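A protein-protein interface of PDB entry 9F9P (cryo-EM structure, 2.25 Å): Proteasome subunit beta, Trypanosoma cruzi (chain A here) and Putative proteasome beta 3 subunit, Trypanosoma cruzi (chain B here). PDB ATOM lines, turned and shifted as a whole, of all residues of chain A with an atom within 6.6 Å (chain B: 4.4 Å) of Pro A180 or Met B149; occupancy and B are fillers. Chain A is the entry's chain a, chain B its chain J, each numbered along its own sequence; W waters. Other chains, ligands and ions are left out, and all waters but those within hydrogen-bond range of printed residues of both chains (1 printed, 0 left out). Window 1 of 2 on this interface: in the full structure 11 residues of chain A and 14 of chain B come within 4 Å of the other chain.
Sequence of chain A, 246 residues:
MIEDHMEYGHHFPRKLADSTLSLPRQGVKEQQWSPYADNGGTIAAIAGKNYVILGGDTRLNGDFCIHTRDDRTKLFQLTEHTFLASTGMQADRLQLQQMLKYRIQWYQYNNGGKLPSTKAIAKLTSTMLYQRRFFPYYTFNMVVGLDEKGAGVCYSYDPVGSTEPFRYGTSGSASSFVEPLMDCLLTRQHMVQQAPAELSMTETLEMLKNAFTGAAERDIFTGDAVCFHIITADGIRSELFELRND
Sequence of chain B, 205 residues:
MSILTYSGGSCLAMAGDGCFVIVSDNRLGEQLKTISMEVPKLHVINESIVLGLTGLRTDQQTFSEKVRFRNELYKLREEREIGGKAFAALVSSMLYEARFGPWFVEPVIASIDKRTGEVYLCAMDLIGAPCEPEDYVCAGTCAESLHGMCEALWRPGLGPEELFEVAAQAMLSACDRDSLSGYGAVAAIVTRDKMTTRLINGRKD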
ATOM      1  N   THR A 170     -28.413  -7.708   2.019  1.00  0.00           N
ATOM      2  CA  THR A 170     -29.817  -7.689   2.390  1.00  0.00           C
ATOM      3  C   THR A 170     -30.144  -6.456   3.213  1.00  0.00           C
ATOM      4  O   THR A 170     -29.288  -5.977   3.938  1.00  0.00           O
ATOM      5  CB  THR A 170     -30.191  -8.981   3.135  1.00  0.00           C
ATOM      6  OG1 THR A 170     -31.523  -8.885   3.654  1.00  0.00           O
ATOM      7  CG2 THR A 170     -29.275  -9.270   4.288  1.00  0.00           C
ATOM      8  N   SER A 175     -33.557  -8.492   7.908  1.00  0.00           N
ATOM      9  CA  SER A 175     -32.201  -8.558   7.405  1.00  0.00           C
ATOM     10  C   SER A 175     -31.242  -9.113   8.454  1.00  0.00           C
ATOM     11  O   SER A 175     -30.291  -9.802   8.117  1.00  0.00           O
ATOM     12  CB  SER A 175     -31.766  -7.230   6.888  1.00  0.00           C
ATOM     13  OG  SER A 175     -31.364  -6.366   7.921  1.00  0.00           O
ATOM     14  N   SER A 176     -31.526  -8.907   9.737  1.00  0.00           N
ATOM     15  CA  SER A 176     -30.688  -9.447  10.807  1.00  0.00           C
ATOM     16  C   SER A 176     -30.825 -10.970  10.944  1.00  0.00           C
ATOM     17  O   SER A 176     -30.002 -11.540  11.638  1.00  0.00           O
ATOM     18  CB  SER A 176     -31.009  -8.786  12.144  1.00  0.00           C
ATOM     19  OG  SER A 176     -32.238  -9.339  12.626  1.00  0.00           O
ATOM     20  N   PHE A 177     -31.866 -11.599  10.372  1.00  0.00           N
ATOM     21  CA  PHE A 177     -31.912 -13.048  10.224  1.00  0.00           C
ATOM     22  C   PHE A 177     -31.103 -13.523   9.026  1.00  0.00           C
ATOM     23  O   PHE A 177     -30.265 -14.412   9.163  1.00  0.00           O
ATOM     24  CB  PHE A 177     -33.277 -13.615   9.809  1.00  0.00           C
ATOM     25  CG  PHE A 177     -34.430 -13.274  10.703  1.00  0.00           C
ATOM     26  CD1 PHE A 177     -34.228 -12.859  12.010  1.00  0.00           C
ATOM     27  CD2 PHE A 177     -35.715 -13.329  10.214  1.00  0.00           C
ATOM     28  CE1 PHE A 177     -35.302 -12.535  12.824  1.00  0.00           C
ATOM     29  CE2 PHE A 177     -36.782 -12.946  11.010  1.00  0.00           C
ATOM     30  CZ  PHE A 177     -36.579 -12.571  12.321  1.00  0.00           C
ATOM     31  N   VAL A 178     -31.401 -12.947   7.850  1.00  0.00           N
ATOM     32  CA  VAL A 178     -30.969 -13.481   6.563  1.00  0.00           C
ATOM     33  C   VAL A 178     -29.451 -13.323   6.415  1.00  0.00           C
ATOM     34  O   VAL A 178     -28.789 -14.134   5.779  1.00  0.00           O
ATOM     35  CB  VAL A 178     -31.743 -12.795   5.418  1.00  0.00           C
ATOM     36  CG1 VAL A 178     -31.278 -13.240   4.040  1.00  0.00           C
ATOM     37  CG2 VAL A 178     -33.231 -13.040   5.527  1.00  0.00           C
ATOM     38  N   GLU A 179     -28.906 -12.244   6.953  1.00  0.00           N
ATOM     39  CA  GLU A 179     -27.515 -11.898   6.717  1.00  0.00           C
ATOM     40  C   GLU A 179     -26.574 -12.899   7.378  1.00  0.00           C
ATOM     41  O   GLU A 179     -25.626 -13.321   6.728  1.00  0.00           O
ATOM     42  CB  GLU A 179     -27.220 -10.477   7.190  1.00  0.00           C
ATOM     43  CG  GLU A 179     -25.924  -9.898   6.633  1.00  0.00           C
ATOM     44  CD  GLU A 179     -25.884  -8.371   6.555  1.00  0.00           C
ATOM     45  OE1 GLU A 179     -25.737  -7.714   7.638  1.00  0.00           O
ATOM     46  OE2 GLU A 179     -26.015  -7.826   5.409  1.00  0.00           O
ATOM     47  N   PRO A 180     -26.707 -13.268   8.680  1.00  0.00           N
ATOM     48  CA  PRO A 180     -25.877 -14.324   9.258  1.00  0.00           C
ATOM     49  C   PRO A 180     -26.007 -15.688   8.584  1.00  0.00           C
ATOM     50  O   PRO A 180     -25.034 -16.426   8.544  1.00  0.00           O
ATOM     51  CB  PRO A 180     -26.254 -14.432  10.743  1.00  0.00           C
ATOM     52  CG  PRO A 180     -27.422 -13.473  10.953  1.00  0.00           C
ATOM     53  CD  PRO A 180     -27.536 -12.620   9.704  1.00  0.00           C
ATOM     54  N   LEU A 181     -27.167 -15.999   8.011  1.00  0.00           N
ATOM     55  CA  LEU A 181     -27.314 -17.247   7.269  1.00  0.00           C
ATOM     56  C   LEU A 181     -26.477 -17.244   5.986  1.00  0.00           C
ATOM     57  O   LEU A 181     -25.773 -18.206   5.736  1.00  0.00           O
ATOM     58  CB  LEU A 181     -28.792 -17.444   6.961  1.00  0.00           C
ATOM     59  CG  LEU A 181     -29.129 -18.733   6.220  1.00  0.00           C
ATOM     60  CD1 LEU A 181     -28.743 -19.928   7.079  1.00  0.00           C
ATOM     61  CD2 LEU A 181     -30.611 -18.782   5.827  1.00  0.00           C
ATOM     62  N   MET A 182     -26.501 -16.142   5.217  1.00  0.00           N
ATOM     63  CA  MET A 182     -25.689 -15.965   4.020  1.00  0.00           C
ATOM     64  C   MET A 182     -24.194 -16.028   4.352  1.00  0.00           C
ATOM     65  O   MET A 182     -23.421 -16.566   3.585  1.00  0.00           O
ATOM     66  CB  MET A 182     -25.960 -14.600   3.366  1.00  0.00           C
ATOM     67  CG  MET A 182     -27.231 -14.522   2.488  1.00  0.00           C
ATOM     68  SD  MET A 182     -27.631 -12.758   2.092  1.00  0.00           S
ATOM     69  CE  MET A 182     -28.682 -12.927   0.669  1.00  0.00           C
ATOM     70  N   ASP A 183     -23.765 -15.423   5.464  1.00  0.00           N
ATOM     71  CA  ASP A 183     -22.384 -15.555   5.903  1.00  0.00           C
ATOM     72  C   ASP A 183     -22.034 -17.031   6.087  1.00  0.00           C
ATOM     73  O   ASP A 183     -20.946 -17.437   5.719  1.00  0.00           O
ATOM     74  CB  ASP A 183     -22.115 -14.832   7.227  1.00  0.00           C
ATOM     75  CG  ASP A 183     -22.242 -13.309   7.234  1.00  0.00           C
ATOM     76  OD1 ASP A 183     -22.088 -12.693   6.159  1.00  0.00           O
ATOM     77  OD2 ASP A 183     -22.509 -12.740   8.321  1.00  0.00           O
ATOM     78  N   CYS A 184     -22.926 -17.810   6.705  1.00  0.00           N
ATOM     79  CA  CYS A 184     -22.671 -19.204   7.050  1.00  0.00           C
ATOM     80  C   CYS A 184     -22.537 -20.013   5.757  1.00  0.00           C
ATOM     81  O   CYS A 184     -21.469 -20.565   5.524  1.00  0.00           O
ATOM     82  CB  CYS A 184     -23.726 -19.811   8.006  1.00  0.00           C
ATOM     83  SG  CYS A 184     -23.341 -21.474   8.671  1.00  0.00           S
ATOM     84  N   LEU A 185     -23.565 -20.021   4.900  1.00  0.00           N
ATOM     85  CA  LEU A 185     -23.585 -20.895   3.728  1.00  0.00           C
ATOM     86  C   LEU A 185     -22.644 -20.445   2.602  1.00  0.00           C
ATOM     87  O   LEU A 185     -22.280 -21.284   1.795  1.00  0.00           O
ATOM     88  CB  LEU A 185     -25.020 -20.993   3.190  1.00  0.00           C
ATOM     89  CG  LEU A 185     -26.083 -21.426   4.208  1.00  0.00           C
ATOM     90  CD1 LEU A 185     -27.475 -21.484   3.577  1.00  0.00           C
ATOM     91  CD2 LEU A 185     -25.716 -22.767   4.856  1.00  0.00           C
ATOM     92  N   SER B 145     -30.613 -12.375  15.632  1.00  0.00           N
ATOM     93  CA  SER B 145     -29.871 -13.204  14.697  1.00  0.00           C
ATOM     94  C   SER B 145     -29.960 -14.675  15.056  1.00  0.00           C
ATOM     95  O   SER B 145     -30.151 -15.480  14.163  1.00  0.00           O
ATOM     96  CB  SER B 145     -28.442 -12.783  14.608  1.00  0.00           C
ATOM     97  OG  SER B 145     -28.379 -11.422  14.214  1.00  0.00           O
ATOM     98  N   LEU B 146     -29.831 -15.025  16.340  1.00  0.00           N
ATOM     99  CA  LEU B 146     -29.872 -16.415  16.787  1.00  0.00           C
ATOM    100  C   LEU B 146     -31.192 -17.066  16.413  1.00  0.00           C
ATOM    101  O   LEU B 146     -31.233 -18.206  15.971  1.00  0.00           O
ATOM    102  CB  LEU B 146     -29.732 -16.481  18.308  1.00  0.00           C
ATOM    103  CG  LEU B 146     -28.351 -16.722  18.890  1.00  0.00           C
ATOM    104  CD1 LEU B 146     -28.405 -16.689  20.406  1.00  0.00           C
ATOM    105  CD2 LEU B 146     -27.797 -18.050  18.424  1.00  0.00           C
ATOM    106  N   HIS B 147     -32.271 -16.320  16.638  1.00  0.00           N
ATOM    107  CA  HIS B 147     -33.633 -16.782  16.400  1.00  0.00           C
ATOM    108  C   HIS B 147     -33.798 -17.179  14.940  1.00  0.00           C
ATOM    109  O   HIS B 147     -34.408 -18.205  14.646  1.00  0.00           O
ATOM    110  CB  HIS B 147     -34.628 -15.726  16.899  1.00  0.00           C
ATOM    111  CG  HIS B 147     -35.907 -16.255  17.440  1.00  0.00           C
ATOM    112  ND1 HIS B 147     -35.994 -16.983  18.621  1.00  0.00           N
ATOM    113  CD2 HIS B 147     -37.164 -16.107  16.965  1.00  0.00           C
ATOM    114  CE1 HIS B 147     -37.270 -17.296  18.817  1.00  0.00           C
ATOM    115  NE2 HIS B 147     -38.006 -16.776  17.823  1.00  0.00           N
ATOM    116  N   GLY B 148     -33.179 -16.418  14.027  1.00  0.00           N
ATOM    117  CA  GLY B 148     -33.204 -16.741  12.598  1.00  0.00           C
ATOM    118  C   GLY B 148     -32.243 -17.848  12.165  1.00  0.00           C
ATOM    119  O   GLY B 148     -32.543 -18.604  11.264  1.00  0.00           O
ATOM    120  N   MET B 149     -31.076 -17.970  12.773  1.00  0.00           N
ATOM    121  CA  MET B 149     -30.203 -19.095  12.454  1.00  0.00           C
ATOM    122  C   MET B 149     -30.821 -20.452  12.816  1.00  0.00           C
ATOM    123  O   MET B 149     -30.669 -21.431  12.074  1.00  0.00           O
ATOM    124  CB  MET B 149     -28.876 -18.979  13.194  1.00  0.00           C
ATOM    125  CG  MET B 149     -27.984 -17.844  12.688  1.00  0.00           C
ATOM    126  SD  MET B 149     -27.585 -17.975  10.936  1.00  0.00           S
ATOM    127  CE  MET B 149     -26.890 -19.628  10.861  1.00  0.00           C
ATOM    128  N   CYS B 150     -31.499 -20.527  13.967  1.00  0.00           N
ATOM    129  CA  CYS B 150     -32.086 -21.780  14.422  1.00  0.00           C
ATOM    130  C   CYS B 150     -33.254 -22.194  13.534  1.00  0.00           C
ATOM    131  O   CYS B 150     -33.350 -23.346  13.168  1.00  0.00           O
ATOM    132  CB  CYS B 150     -32.554 -21.686  15.867  1.00  0.00           C
ATOM    133  SG  CYS B 150     -31.246 -21.284  17.056  1.00  0.00           S
ATOM    134  N   GLU B 151     -34.117 -21.252  13.163  1.00  0.00           N
ATOM    135  CA  GLU B 151     -35.212 -21.527  12.244  1.00  0.00           C
ATOM    136  C   GLU B 151     -34.714 -22.134  10.926  1.00  0.00           C
ATOM    137  O   GLU B 151     -35.419 -22.917  10.307  1.00  0.00           O
ATOM    138  CB  GLU B 151     -36.004 -20.240  11.979  1.00  0.00           C
ATOM    139  CG  GLU B 151     -37.169 -20.356  10.986  1.00  0.00           C
ATOM    140  CD  GLU B 151     -38.358 -21.215  11.412  1.00  0.00           C
ATOM    141  OE1 GLU B 151     -38.993 -21.855  10.516  1.00  0.00           O
ATOM    142  OE2 GLU B 151     -38.638 -21.281  12.646  1.00  0.00           O
ATOM    143  N   ALA B 152     -33.511 -21.759  10.481  1.00  0.00           N
ATOM    144  CA  ALA B 152     -32.974 -22.268   9.226  1.00  0.00           C
ATOM    145  C   ALA B 152     -32.295 -23.633   9.358  1.00  0.00           C
ATOM    146  O   ALA B 152     -32.360 -24.377   8.404  1.00  0.00           O
ATOM    147  CB  ALA B 152     -32.022 -21.258   8.652  1.00  0.00           C
ATOM    148  N   LEU B 153     -31.611 -23.936  10.484  1.00  0.00           N
ATOM    149  CA  LEU B 153     -30.754 -25.123  10.611  1.00  0.00           C
ATOM    150  C   LEU B 153     -31.411 -26.248  11.413  1.00  0.00           C
ATOM    151  O   LEU B 153     -31.041 -27.403  11.263  1.00  0.00           O
ATOM    152  CB  LEU B 153     -29.424 -24.760  11.289  1.00  0.00           C
ATOM    153  CG  LEU B 153     -28.607 -23.594  10.694  1.00  0.00           C
ATOM    154  CD1 LEU B 153     -27.319 -23.313  11.486  1.00  0.00           C
ATOM    155  CD2 LEU B 153     -28.262 -23.826   9.228  1.00  0.00           C
ATOM    156  N   ALA B 170     -24.922 -22.120  14.754  1.00  0.00           N
ATOM    157  CA  ALA B 170     -25.855 -21.039  14.965  1.00  0.00           C
ATOM    158  C   ALA B 170     -25.242 -20.006  15.913  1.00  0.00           C
ATOM    159  O   ALA B 170     -25.392 -18.801  15.699  1.00  0.00           O
ATOM    160  CB  ALA B 170     -27.168 -21.550  15.531  1.00  0.00           C
ATOM    161  N   SER B 173     -22.220 -18.014  14.035  1.00  0.00           N
ATOM    162  CA  SER B 173     -22.645 -17.071  13.023  1.00  0.00           C
ATOM    163  C   SER B 173     -23.308 -15.845  13.637  1.00  0.00           C
ATOM    164  O   SER B 173     -23.112 -14.734  13.169  1.00  0.00           O
ATOM    165  CB  SER B 173     -23.573 -17.719  12.046  1.00  0.00           C
ATOM    166  OG  SER B 173     -22.976 -18.914  11.595  1.00  0.00           O
HETATM  167  O   HOH W   1     -21.900 -14.093  10.692  1.00  0.00           O
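Ser A175 touches none of the printed residues of chain B.
Printed residues of chain B within 4 Å of Ser A176: Ser B145 (3.0 Å).
Printed residues of chain B within 4 Å of Pro A180: Ser B145, Met B149 and Ser B173.
Of the printed residues of chain B, Leu A181 touches Met B149 (3.6 Å) and Ala B152 (3.9 Å).
Of the printed residues of chain B, Cys A184 touches Ser B173 (3.8 Å).
Printed residues of chain A within 4 Å of Ser B145: Ser A176 and Pro A180.
Printed residues of chain A within 4 Å of Ala B152: Leu A181.
The nearest residue of chain A that does not touch Met B149 is Cys A184 (4.3 Å).
Printed residues of chain B that touch a printed residue of chain A: Ser B145, Met B149, Ala B152 and Ser B173.
Hydrophobic or aromatic side chains of chain B that line the printed part of chain A: Met B149 and Ala B152.
Of the 12 printed residues of chain A, 4 touch a printed residue of chain B.
Hydrophobic or aromatic side chains of chain A within 4 Å of the printed part of chain B: Pro A180 and Leu A181.
Among the printed residues, no Asp or Glu carboxylate lies within 4 Å of a Lys or Arg side-chain nitrogen of the other chain.
Water W1 lies within hydrogen-bond range of OD2 of Asp A183 (2.8 Å) and O of Ser B173 (2.8 Å).
The side-chain hydroxyl (OG) of Ser B145 lies within hydrogen-bond range of the backbone carbonyl oxygen (O) of Ser A176.
The side-chain sulfur (SD) of Met B149 lies within hydrogen-bond range of the backbone NH (N) of Leu A181 (3.6 Å).
Pro A180 touches Ser B145.
Pro A180 touches Met B149 (C to SD, 3.6 Å).
Ser B173 touches Pro A180 (O to CB, 3.98 Å).
Leu A181 touches Ala B152 (CD1 to CB, 3.9 Å).
CB of Cys A184 touches OG of Ser B173 (3.8 Å).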
